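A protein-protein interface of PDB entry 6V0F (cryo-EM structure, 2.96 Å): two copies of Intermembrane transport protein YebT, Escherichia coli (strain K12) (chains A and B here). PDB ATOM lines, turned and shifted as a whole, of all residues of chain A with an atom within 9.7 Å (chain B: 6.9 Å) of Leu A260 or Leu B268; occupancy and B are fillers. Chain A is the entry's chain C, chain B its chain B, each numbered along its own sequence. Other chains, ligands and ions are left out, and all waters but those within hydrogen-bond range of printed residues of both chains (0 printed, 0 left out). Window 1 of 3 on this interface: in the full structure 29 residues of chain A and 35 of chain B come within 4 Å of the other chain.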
ATOM      1  N   PRO A 254      19.045  31.201 -16.819  1.00  0.00           N
ATOM      2  CA  PRO A 254      17.777  30.485 -16.693  1.00  0.00           C
ATOM      3  C   PRO A 254      17.969  28.994 -16.475  1.00  0.00           C
ATOM      4  O   PRO A 254      19.035  28.434 -16.711  1.00  0.00           O
ATOM      5  CB  PRO A 254      17.123  30.729 -18.054  1.00  0.00           C
ATOM      6  CG  PRO A 254      18.272  30.808 -18.968  1.00  0.00           C
ATOM      7  CD  PRO A 254      19.392  31.450 -18.223  1.00  0.00           C
ATOM      8  N   LEU A 255      16.900  28.357 -16.011  1.00  0.00           N
ATOM      9  CA  LEU A 255      16.812  26.904 -15.973  1.00  0.00           C
ATOM     10  C   LEU A 255      15.892  26.469 -17.102  1.00  0.00           C
ATOM     11  O   LEU A 255      14.673  26.611 -16.999  1.00  0.00           O
ATOM     12  CB  LEU A 255      16.278  26.422 -14.629  1.00  0.00           C
ATOM     13  CG  LEU A 255      16.083  24.914 -14.477  1.00  0.00           C
ATOM     14  CD1 LEU A 255      17.397  24.199 -14.544  1.00  0.00           C
ATOM     15  CD2 LEU A 255      15.367  24.557 -13.203  1.00  0.00           C
ATOM     16  N   MET A 256      16.463  25.914 -18.162  1.00  0.00           N
ATOM     17  CA  MET A 256      15.661  25.420 -19.268  1.00  0.00           C
ATOM     18  C   MET A 256      15.089  24.053 -18.946  1.00  0.00           C
ATOM     19  O   MET A 256      15.749  23.218 -18.331  1.00  0.00           O
ATOM     20  CB  MET A 256      16.483  25.310 -20.544  1.00  0.00           C
ATOM     21  CG  MET A 256      16.858  26.584 -21.265  1.00  0.00           C
ATOM     22  SD  MET A 256      15.535  27.558 -21.986  1.00  0.00           S
ATOM     23  CE  MET A 256      15.669  29.043 -21.025  1.00  0.00           C
ATOM     24  N   TYR A 257      13.858  23.823 -19.379  1.00  0.00           N
ATOM     25  CA  TYR A 257      13.300  22.480 -19.427  1.00  0.00           C
ATOM     26  C   TYR A 257      12.427  22.398 -20.660  1.00  0.00           C
ATOM     27  O   TYR A 257      11.549  23.244 -20.841  1.00  0.00           O
ATOM     28  CB  TYR A 257      12.506  22.142 -18.173  1.00  0.00           C
ATOM     29  CG  TYR A 257      11.806  20.816 -18.268  1.00  0.00           C
ATOM     30  CD1 TYR A 257      12.526  19.639 -18.305  1.00  0.00           C
ATOM     31  CD2 TYR A 257      10.429  20.739 -18.282  1.00  0.00           C
ATOM     32  CE1 TYR A 257      11.898  18.428 -18.389  1.00  0.00           C
ATOM     33  CE2 TYR A 257       9.791  19.530 -18.361  1.00  0.00           C
ATOM     34  CZ  TYR A 257      10.532  18.380 -18.413  1.00  0.00           C
ATOM     35  OH  TYR A 257       9.898  17.170 -18.490  1.00  0.00           O
ATOM     36  N   GLN A 258      12.737  21.434 -21.535  1.00  0.00           N
ATOM     37  CA  GLN A 258      12.102  21.249 -22.845  1.00  0.00           C
ATOM     38  C   GLN A 258      12.213  22.502 -23.702  1.00  0.00           C
ATOM     39  O   GLN A 258      11.342  22.789 -24.519  1.00  0.00           O
ATOM     40  CB  GLN A 258      10.636  20.829 -22.719  1.00  0.00           C
ATOM     41  CG  GLN A 258      10.405  19.475 -22.091  1.00  0.00           C
ATOM     42  CD  GLN A 258      11.015  18.354 -22.882  1.00  0.00           C
ATOM     43  OE1 GLN A 258      11.973  17.723 -22.444  1.00  0.00           O
ATOM     44  NE2 GLN A 258      10.463  18.092 -24.057  1.00  0.00           N
ATOM     45  N   GLY A 259      13.286  23.258 -23.515  1.00  0.00           N
ATOM     46  CA  GLY A 259      13.501  24.473 -24.255  1.00  0.00           C
ATOM     47  C   GLY A 259      12.786  25.683 -23.708  1.00  0.00           C
ATOM     48  O   GLY A 259      12.869  26.751 -24.318  1.00  0.00           O
ATOM     49  N   LEU A 260      12.127  25.574 -22.561  1.00  0.00           N
ATOM     50  CA  LEU A 260      11.385  26.694 -22.009  1.00  0.00           C
ATOM     51  C   LEU A 260      12.024  27.184 -20.723  1.00  0.00           C
ATOM     52  O   LEU A 260      12.616  26.409 -19.973  1.00  0.00           O
ATOM     53  CB  LEU A 260       9.932  26.317 -21.752  1.00  0.00           C
ATOM     54  CG  LEU A 260       9.200  26.020 -23.047  1.00  0.00           C
ATOM     55  CD1 LEU A 260       7.832  25.528 -22.762  1.00  0.00           C
ATOM     56  CD2 LEU A 260       9.124  27.278 -23.851  1.00  0.00           C
ATOM     57  N   GLU A 261      11.893  28.484 -20.476  1.00  0.00           N
ATOM     58  CA  GLU A 261      12.455  29.075 -19.273  1.00  0.00           C
ATOM     59  C   GLU A 261      11.580  28.735 -18.086  1.00  0.00           C
ATOM     60  O   GLU A 261      10.402  29.098 -18.036  1.00  0.00           O
ATOM     61  CB  GLU A 261      12.619  30.582 -19.417  1.00  0.00           C
ATOM     62  CG  GLU A 261      13.321  31.201 -18.230  1.00  0.00           C
ATOM     63  CD  GLU A 261      13.572  32.675 -18.408  1.00  0.00           C
ATOM     64  OE1 GLU A 261      13.184  33.221 -19.461  1.00  0.00           O
ATOM     65  OE2 GLU A 261      14.153  33.292 -17.491  1.00  0.00           O
ATOM     66  N   VAL A 262      12.177  28.049 -17.131  1.00  0.00           N
ATOM     67  CA  VAL A 262      11.508  27.458 -15.989  1.00  0.00           C
ATOM     68  C   VAL A 262      11.989  28.091 -14.698  1.00  0.00           C
ATOM     69  O   VAL A 262      11.217  28.306 -13.757  1.00  0.00           O
ATOM     70  CB  VAL A 262      11.779  25.949 -16.034  1.00  0.00           C
ATOM     71  CG1 VAL A 262      11.380  25.318 -14.821  1.00  0.00           C
ATOM     72  CG2 VAL A 262      10.964  25.340 -17.148  1.00  0.00           C
ATOM     73  N   GLY A 263      13.241  28.493 -14.687  1.00  0.00           N
ATOM     74  CA  GLY A 263      13.828  29.022 -13.486  1.00  0.00           C
ATOM     75  C   GLY A 263      14.670  30.230 -13.779  1.00  0.00           C
ATOM     76  O   GLY A 263      14.704  30.724 -14.905  1.00  0.00           O
ATOM     77  N   GLN A 264      15.344  30.721 -12.756  1.00  0.00           N
ATOM     78  CA  GLN A 264      16.159  31.914 -12.881  1.00  0.00           C
ATOM     79  C   GLN A 264      17.154  31.805 -11.746  1.00  0.00           C
ATOM     80  O   GLN A 264      16.737  31.647 -10.597  1.00  0.00           O
ATOM     81  CB  GLN A 264      15.298  33.158 -12.744  1.00  0.00           C
ATOM     82  CG  GLN A 264      15.969  34.461 -13.060  1.00  0.00           C
ATOM     83  CD  GLN A 264      16.298  34.579 -14.530  1.00  0.00           C
ATOM     84  OE1 GLN A 264      17.454  34.482 -14.931  1.00  0.00           O
ATOM     85  NE2 GLN A 264      15.276  34.788 -15.346  1.00  0.00           N
ATOM     86  N   VAL A 282      12.333  28.363  -8.931  1.00  0.00           N
ATOM     87  CA  VAL A 282      11.581  27.695  -9.986  1.00  0.00           C
ATOM     88  C   VAL A 282      10.096  27.937  -9.748  1.00  0.00           C
ATOM     89  O   VAL A 282       9.663  28.169  -8.614  1.00  0.00           O
ATOM     90  CB  VAL A 282      11.903  26.190 -10.046  1.00  0.00           C
ATOM     91  CG1 VAL A 282      13.348  25.991 -10.373  1.00  0.00           C
ATOM     92  CG2 VAL A 282      11.604  25.532  -8.736  1.00  0.00           C
ATOM     93  N   ASP A 283       9.309  27.908 -10.827  1.00  0.00           N
ATOM     94  CA  ASP A 283       7.873  28.110 -10.694  1.00  0.00           C
ATOM     95  C   ASP A 283       7.236  26.835 -10.115  1.00  0.00           C
ATOM     96  O   ASP A 283       7.877  25.786 -10.089  1.00  0.00           O
ATOM     97  CB  ASP A 283       7.306  28.576 -12.043  1.00  0.00           C
ATOM     98  CG  ASP A 283       7.617  27.646 -13.166  1.00  0.00           C
ATOM     99  OD1 ASP A 283       8.394  26.708 -12.951  1.00  0.00           O
ATOM    100  OD2 ASP A 283       7.087  27.862 -14.274  1.00  0.00           O
ATOM    101  N   SER A 285       4.825  24.654 -11.124  1.00  0.00           N
ATOM    102  CA  SER A 285       4.526  23.541 -12.030  1.00  0.00           C
ATOM    103  C   SER A 285       5.558  22.403 -12.008  1.00  0.00           C
ATOM    104  O   SER A 285       5.250  21.263 -11.650  1.00  0.00           O
ATOM    105  CB  SER A 285       4.378  24.087 -13.449  1.00  0.00           C
ATOM    106  OG  SER A 285       5.615  24.572 -13.935  1.00  0.00           O
ATOM    107  N   VAL A 286       6.794  22.720 -12.394  1.00  0.00           N
ATOM    108  CA  VAL A 286       7.978  21.856 -12.325  1.00  0.00           C
ATOM    109  C   VAL A 286       8.346  21.334 -10.945  1.00  0.00           C
ATOM    110  O   VAL A 286       9.184  20.433 -10.859  1.00  0.00           O
ATOM    111  CB  VAL A 286       9.175  22.552 -12.955  1.00  0.00           C
ATOM    112  CG1 VAL A 286       8.875  22.767 -14.418  1.00  0.00           C
ATOM    113  CG2 VAL A 286       9.497  23.779 -12.182  1.00  0.00           C
ATOM    114  N   THR A 318      23.819  27.757 -19.481  1.00  0.00           N
ATOM    115  CA  THR A 318      22.390  27.482 -19.449  1.00  0.00           C
ATOM    116  C   THR A 318      22.140  26.246 -18.610  1.00  0.00           C
ATOM    117  O   THR A 318      22.595  25.164 -18.963  1.00  0.00           O
ATOM    118  CB  THR A 318      21.848  27.296 -20.858  1.00  0.00           C
ATOM    119  OG1 THR A 318      21.969  28.523 -21.583  1.00  0.00           O
ATOM    120  CG2 THR A 318      20.422  26.894 -20.811  1.00  0.00           C
ATOM    121  N   PHE A 319      21.370  26.384 -17.550  1.00  0.00           N
ATOM    122  CA  PHE A 319      21.064  25.254 -16.690  1.00  0.00           C
ATOM    123  C   PHE A 319      19.975  24.398 -17.312  1.00  0.00           C
ATOM    124  O   PHE A 319      18.877  24.883 -17.592  1.00  0.00           O
ATOM    125  CB  PHE A 319      20.631  25.769 -15.329  1.00  0.00           C
ATOM    126  CG  PHE A 319      21.749  26.258 -14.494  1.00  0.00           C
ATOM    127  CD1 PHE A 319      22.986  25.680 -14.579  1.00  0.00           C
ATOM    128  CD2 PHE A 319      21.585  27.353 -13.684  1.00  0.00           C
ATOM    129  CE1 PHE A 319      24.014  26.137 -13.810  1.00  0.00           C
ATOM    130  CE2 PHE A 319      22.606  27.815 -12.922  1.00  0.00           C
ATOM    131  CZ  PHE A 319      23.820  27.208 -12.987  1.00  0.00           C
ATOM    132  N   GLU A 320      20.287  23.135 -17.549  1.00  0.00           N
ATOM    133  CA  GLU A 320      19.341  22.177 -18.093  1.00  0.00           C
ATOM    134  C   GLU A 320      18.857  21.255 -16.988  1.00  0.00           C
ATOM    135  O   GLU A 320      19.661  20.735 -16.200  1.00  0.00           O
ATOM    136  CB  GLU A 320      19.982  21.360 -19.212  1.00  0.00           C
ATOM    137  CG  GLU A 320      19.090  20.291 -19.831  1.00  0.00           C
ATOM    138  CD  GLU A 320      17.952  20.848 -20.656  1.00  0.00           C
ATOM    139  OE1 GLU A 320      18.088  21.961 -21.202  1.00  0.00           O
ATOM    140  OE2 GLU A 320      16.916  20.161 -20.767  1.00  0.00           O
ATOM    141  N   LEU A 321      17.548  21.059 -16.943  1.00  0.00           N
ATOM    142  CA  LEU A 321      16.890  20.193 -15.982  1.00  0.00           C
ATOM    143  C   LEU A 321      16.521  18.890 -16.666  1.00  0.00           C
ATOM    144  O   LEU A 321      15.826  18.903 -17.684  1.00  0.00           O
ATOM    145  CB  LEU A 321      15.629  20.855 -15.440  1.00  0.00           C
ATOM    146  CG  LEU A 321      14.857  20.024 -14.425  1.00  0.00           C
ATOM    147  CD1 LEU A 321      15.699  19.787 -13.213  1.00  0.00           C
ATOM    148  CD2 LEU A 321      13.563  20.690 -14.048  1.00  0.00           C
ATOM    149  N   LEU B 242       4.154  20.863 -30.207  1.00  0.00           N
ATOM    150  CA  LEU B 242       5.535  21.162 -30.536  1.00  0.00           C
ATOM    151  C   LEU B 242       6.470  20.106 -29.954  1.00  0.00           C
ATOM    152  O   LEU B 242       6.145  19.472 -28.951  1.00  0.00           O
ATOM    153  CB  LEU B 242       5.902  22.536 -30.006  1.00  0.00           C
ATOM    154  CG  LEU B 242       5.059  23.592 -30.705  1.00  0.00           C
ATOM    155  CD1 LEU B 242       5.183  24.907 -30.019  1.00  0.00           C
ATOM    156  CD2 LEU B 242       5.481  23.701 -32.137  1.00  0.00           C
ATOM    157  N   SER B 244       9.772  20.830 -28.916  1.00  0.00           N
ATOM    158  CA  SER B 244      10.374  21.599 -27.845  1.00  0.00           C
ATOM    159  C   SER B 244      10.186  23.067 -28.174  1.00  0.00           C
ATOM    160  O   SER B 244       9.904  23.432 -29.314  1.00  0.00           O
ATOM    161  CB  SER B 244      11.854  21.268 -27.668  1.00  0.00           C
ATOM    162  OG  SER B 244      12.611  21.779 -28.742  1.00  0.00           O
ATOM    163  N   GLY B 245      10.357  23.909 -27.170  1.00  0.00           N
ATOM    164  CA  GLY B 245      10.202  25.335 -27.357  1.00  0.00           C
ATOM    165  C   GLY B 245      11.552  26.008 -27.352  1.00  0.00           C
ATOM    166  O   GLY B 245      11.684  27.143 -26.886  1.00  0.00           O
ATOM    167  N   ALA B 246      12.554  25.286 -27.867  1.00  0.00           N
ATOM    168  CA  ALA B 246      13.951  25.707 -27.804  1.00  0.00           C
ATOM    169  C   ALA B 246      14.208  27.055 -28.462  1.00  0.00           C
ATOM    170  O   ALA B 246      14.917  27.894 -27.899  1.00  0.00           O
ATOM    171  CB  ALA B 246      14.827  24.639 -28.449  1.00  0.00           C
ATOM    172  N   GLY B 247      13.636  27.302 -29.625  1.00  0.00           N
ATOM    173  CA  GLY B 247      13.873  28.598 -30.225  1.00  0.00           C
ATOM    174  C   GLY B 247      12.585  29.307 -30.550  1.00  0.00           C
ATOM    175  O   GLY B 247      12.573  30.326 -31.241  1.00  0.00           O
ATOM    176  N   LEU B 248      11.489  28.769 -30.044  1.00  0.00           N
ATOM    177  CA  LEU B 248      10.174  29.302 -30.325  1.00  0.00           C
ATOM    178  C   LEU B 248       9.801  30.342 -29.286  1.00  0.00           C
ATOM    179  O   LEU B 248      10.189  30.248 -28.121  1.00  0.00           O
ATOM    180  CB  LEU B 248       9.154  28.171 -30.325  1.00  0.00           C
ATOM    181  CG  LEU B 248       9.532  27.073 -31.307  1.00  0.00           C
ATOM    182  CD1 LEU B 248       8.553  25.942 -31.221  1.00  0.00           C
ATOM    183  CD2 LEU B 248       9.608  27.609 -32.703  1.00  0.00           C
ATOM    184  N   THR B 249       9.065  31.355 -29.721  1.00  0.00           N
ATOM    185  CA  THR B 249       8.794  32.509 -28.889  1.00  0.00           C
ATOM    186  C   THR B 249       7.299  32.796 -28.979  1.00  0.00           C
ATOM    187  O   THR B 249       6.623  32.351 -29.905  1.00  0.00           O
ATOM    188  CB  THR B 249       9.653  33.699 -29.350  1.00  0.00           C
ATOM    189  OG1 THR B 249      10.985  33.237 -29.579  1.00  0.00           O
ATOM    190  CG2 THR B 249       9.777  34.769 -28.278  1.00  0.00           C
ATOM    191  N   ALA B 250       6.786  33.554 -28.027  1.00  0.00           N
ATOM    192  CA  ALA B 250       5.399  33.984 -28.019  1.00  0.00           C
ATOM    193  C   ALA B 250       5.325  35.324 -28.732  1.00  0.00           C
ATOM    194  O   ALA B 250       6.020  36.266 -28.338  1.00  0.00           O
ATOM    195  CB  ALA B 250       4.869  34.088 -26.594  1.00  0.00           C
ATOM    196  N   THR B 253       7.423  34.140 -33.400  1.00  0.00           N
ATOM    197  CA  THR B 253       7.712  33.070 -34.343  1.00  0.00           C
ATOM    198  C   THR B 253       6.660  33.055 -35.435  1.00  0.00           C
ATOM    199  O   THR B 253       5.477  32.856 -35.131  1.00  0.00           O
ATOM    200  CB  THR B 253       7.752  31.726 -33.635  1.00  0.00           C
ATOM    201  OG1 THR B 253       8.782  31.747 -32.646  1.00  0.00           O
ATOM    202  CG2 THR B 253       8.070  30.637 -34.614  1.00  0.00           C
ATOM    203  N   LEU B 265       3.098  32.642 -33.917  1.00  0.00           N
ATOM    204  CA  LEU B 265       2.908  31.790 -32.753  1.00  0.00           C
ATOM    205  C   LEU B 265       2.501  32.656 -31.576  1.00  0.00           C
ATOM    206  O   LEU B 265       3.302  33.452 -31.090  1.00  0.00           O
ATOM    207  CB  LEU B 265       4.192  31.031 -32.434  1.00  0.00           C
ATOM    208  CG  LEU B 265       4.128  30.019 -31.297  1.00  0.00           C
ATOM    209  CD1 LEU B 265       3.183  28.918 -31.650  1.00  0.00           C
ATOM    210  CD2 LEU B 265       5.480  29.449 -31.025  1.00  0.00           C
ATOM    211  N   THR B 266       1.280  32.474 -31.081  1.00  0.00           N
ATOM    212  CA  THR B 266       0.782  33.387 -30.067  1.00  0.00           C
ATOM    213  C   THR B 266       0.843  32.828 -28.661  1.00  0.00           C
ATOM    214  O   THR B 266       0.673  33.596 -27.712  1.00  0.00           O
ATOM    215  CB  THR B 266      -0.657  33.807 -30.365  1.00  0.00           C
ATOM    216  OG1 THR B 266      -1.494  32.654 -30.440  1.00  0.00           O
ATOM    217  CG2 THR B 266      -0.714  34.558 -31.660  1.00  0.00           C
ATOM    218  N   LYS B 267       1.100  31.538 -28.487  1.00  0.00           N
ATOM    219  CA  LYS B 267       1.115  31.027 -27.125  1.00  0.00           C
ATOM    220  C   LYS B 267       2.022  29.814 -27.097  1.00  0.00           C
ATOM    221  O   LYS B 267       2.044  29.027 -28.045  1.00  0.00           O
ATOM    222  CB  LYS B 267      -0.285  30.686 -26.613  1.00  0.00           C
ATOM    223  CG  LYS B 267      -0.350  30.469 -25.120  1.00  0.00           C
ATOM    224  CD  LYS B 267      -1.762  30.291 -24.624  1.00  0.00           C
ATOM    225  CE  LYS B 267      -1.765  30.179 -23.109  1.00  0.00           C
ATOM    226  NZ  LYS B 267      -3.125  29.988 -22.544  1.00  0.00           N
ATOM    227  N   LEU B 268       2.734  29.650 -25.990  1.00  0.00           N
ATOM    228  CA  LEU B 268       3.706  28.581 -25.841  1.00  0.00           C
ATOM    229  C   LEU B 268       3.665  28.110 -24.400  1.00  0.00           C
ATOM    230  O   LEU B 268       4.010  28.863 -23.489  1.00  0.00           O
ATOM    231  CB  LEU B 268       5.088  29.101 -26.218  1.00  0.00           C
ATOM    232  CG  LEU B 268       6.312  28.216 -26.242  1.00  0.00           C
ATOM    233  CD1 LEU B 268       6.124  27.137 -27.249  1.00  0.00           C
ATOM    234  CD2 LEU B 268       7.458  29.090 -26.638  1.00  0.00           C
ATOM    235  N   ASP B 269       3.257  26.864 -24.201  1.00  0.00           N
ATOM    236  CA  ASP B 269       3.011  26.304 -22.885  1.00  0.00           C
ATOM    237  C   ASP B 269       3.809  25.029 -22.697  1.00  0.00           C
ATOM    238  O   ASP B 269       4.109  24.305 -23.652  1.00  0.00           O
ATOM    239  CB  ASP B 269       1.531  25.978 -22.679  1.00  0.00           C
ATOM    240  CG  ASP B 269       0.675  27.207 -22.534  1.00  0.00           C
ATOM    241  OD1 ASP B 269       1.183  28.228 -22.028  1.00  0.00           O
ATOM    242  OD2 ASP B 269      -0.506  27.149 -22.931  1.00  0.00           O
ATOM    243  N   LEU B 270       4.064  24.721 -21.435  1.00  0.00           N
ATOM    244  CA  LEU B 270       4.669  23.460 -21.038  1.00  0.00           C
ATOM    245  C   LEU B 270       3.608  22.706 -20.254  1.00  0.00           C
ATOM    246  O   LEU B 270       3.424  22.929 -19.056  1.00  0.00           O
ATOM    247  CB  LEU B 270       5.921  23.705 -20.207  1.00  0.00           C
ATOM    248  CG  LEU B 270       6.919  22.580 -19.961  1.00  0.00           C
ATOM    249  CD1 LEU B 270       8.261  23.212 -19.809  1.00  0.00           C
ATOM    250  CD2 LEU B 270       6.606  21.798 -18.716  1.00  0.00           C
ATOM    251  N   ASN B 271       2.899  21.832 -20.949  1.00  0.00           N
ATOM    252  CA  ASN B 271       1.913  20.988 -20.315  1.00  0.00           C
ATOM    253  C   ASN B 271       2.615  19.928 -19.468  1.00  0.00           C
ATOM    254  O   ASN B 271       3.751  19.538 -19.777  1.00  0.00           O
ATOM    255  CB  ASN B 271       1.038  20.348 -21.384  1.00  0.00           C
ATOM    256  CG  ASN B 271       0.156  21.352 -22.065  1.00  0.00           C
ATOM    257  OD1 ASN B 271      -0.375  22.256 -21.429  1.00  0.00           O
ATOM    258  ND2 ASN B 271      -0.006  21.208 -23.363  1.00  0.00           N
ATOM    259  N   LYS B 275       5.198  18.154 -22.070  1.00  0.00           N
ATOM    260  CA  LYS B 275       4.618  18.235 -23.409  1.00  0.00           C
ATOM    261  C   LYS B 275       4.399  19.696 -23.766  1.00  0.00           C
ATOM    262  O   LYS B 275       3.414  20.304 -23.343  1.00  0.00           O
ATOM    263  CB  LYS B 275       3.313  17.453 -23.489  1.00  0.00           C
ATOM    264  CG  LYS B 275       3.475  15.977 -23.221  1.00  0.00           C
ATOM    265  CD  LYS B 275       4.319  15.320 -24.289  1.00  0.00           C
ATOM    266  CE  LYS B 275       3.582  15.224 -25.604  1.00  0.00           C
ATOM    267  NZ  LYS B 275       4.397  14.493 -26.608  1.00  0.00           N
ATOM    268  N   VAL B 276       5.302  20.250 -24.565  1.00  0.00           N
ATOM    269  CA  VAL B 276       5.202  21.643 -24.978  1.00  0.00           C
ATOM    270  C   VAL B 276       4.181  21.762 -26.094  1.00  0.00           C
ATOM    271  O   VAL B 276       4.317  21.125 -27.141  1.00  0.00           O
ATOM    272  CB  VAL B 276       6.562  22.179 -25.425  1.00  0.00           C
ATOM    273  CG1 VAL B 276       6.413  23.576 -25.932  1.00  0.00           C
ATOM    274  CG2 VAL B 276       7.519  22.140 -24.279  1.00  0.00           C
ATOM    275  N   THR B 277       3.144  22.559 -25.869  1.00  0.00           N
ATOM    276  CA  THR B 277       2.132  22.820 -26.882  1.00  0.00           C
ATOM    277  C   THR B 277       1.955  24.318 -27.003  1.00  0.00           C
ATOM    278  O   THR B 277       2.017  25.030 -26.005  1.00  0.00           O
ATOM    279  CB  THR B 277       0.783  22.187 -26.552  1.00  0.00           C
ATOM    280  OG1 THR B 277       0.324  22.672 -25.285  1.00  0.00           O
ATOM    281  CG2 THR B 277       0.869  20.665 -26.544  1.00  0.00           C
ATOM    282  N   GLY B 278       1.705  24.796 -28.214  1.00  0.00           N
ATOM    283  CA  GLY B 278       1.468  26.209 -28.415  1.00  0.00           C
ATOM    284  C   GLY B 278       0.311  26.411 -29.365  1.00  0.00           C
ATOM    285  O   GLY B 278      -0.325  25.452 -29.789  1.00  0.00           O
ATOM    286  N   GLU B 279       0.010  27.672 -29.651  1.00  0.00           N
ATOM    287  CA  GLU B 279      -1.076  27.942 -30.576  1.00  0.00           C
ATOM    288  C   GLU B 279      -0.750  29.190 -31.373  1.00  0.00           C
ATOM    289  O   GLU B 279       0.040  30.042 -30.946  1.00  0.00           O
ATOM    290  CB  GLU B 279      -2.421  28.076 -29.868  1.00  0.00           C
ATOM    291  CG  GLU B 279      -2.568  29.296 -29.033  1.00  0.00           C
ATOM    292  CD  GLU B 279      -3.845  29.295 -28.231  1.00  0.00           C
ATOM    293  OE1 GLU B 279      -4.582  28.288 -28.291  1.00  0.00           O
ATOM    294  OE2 GLU B 279      -4.112  30.298 -27.539  1.00  0.00           O
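The backbone NH (N) of Leu B242 sits at hydrogen-bond distance from the backbone carbonyl oxygen (O) of Val B276.
The backbone carbonyl oxygen (O) of Gln A258 sits at hydrogen-bond distance from the backbone NH (N) of Gly B245, at 3.0 Å.
The backbone carbonyl oxygen (O) of Gly B245 sits close to the backbone carbonyl oxygen (O) of Gly A259, at 2.9 Å.
Of the printed residues of chain B, Leu A260 touches Gly B245 (3.97 Å), Leu B268 (3.7 Å), Leu B270 (3.7 Å) and Val B276 (3.7 Å).
Leu B268 touches just one residue of chain A: Leu A260.
Of the printed residues of chain B, Gly A259 touches Gly B245 (2.9 Å) and Ala B246 (3.8 Å).
Of chain A, only Gln A258 (3.0 Å), Gly A259 (2.9 Å) and Leu A260 (3.97 Å) come within 4 Å of Gly B245.
Of the printed residues of chain B, Gln A258 touches Ser B244, Gly B245 and Val B276.
Printed residues of chain A within 4 Å of Val B276: Gln A258 (3.7 Å) and Leu A260 (3.7 Å).
Val A282 touches none of the printed residues of chain B.
The nearest printed residue of chain B that does not touch Leu A260 is Asp B269 (4.02 Å).
The nearest printed residue of chain A that does not touch Leu B270 is Val A262 (4.3 Å).
Of the 21 printed residues of chain B, 6 touch a printed residue of chain A.
Printed residues of chain B that touch a printed residue of chain A: Ser B244, Gly B245, Ala B246, Leu B268, Leu B270 and Val B276.
Hydrophobic or aromatic side chains of chain B that line the printed part of chain A: Leu B268, Leu B270 and Val B276.
Printed residues of chain A that touch a printed residue of chain B: Tyr A257, Gln A258, Gly A259 and Leu A260.
Among the printed residues, 10 pairs touch across the chains.
Among the printed residues, no Asp or Glu carboxylate lies within 4 Å of a Lys or Arg side-chain nitrogen of the other chain.
No position is printed for both chains.
Of the 10 pairs that touch across the chains among the printed residues, none has its exchanged pair printed and touching as well.
CD1 of Leu B270 touches O of Tyr A257, 3.4 Å away.
Ser B244 touches Gln A258.
Gln A258 touches Val B276 (CB to CG2, 3.7 Å).
CA of Gly A259 touches CA of Ala B246, at 3.8 Å.
CD2 of Leu A260 touches O of Gly B245, at 3.97 Å.
Leu B268 touches Leu A260.
CD1 of Leu A260 touches CB of Leu B270, at 3.7 Å.
Leu A260 touches Val B276 (CD1 to CG2, 3.7 Å).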
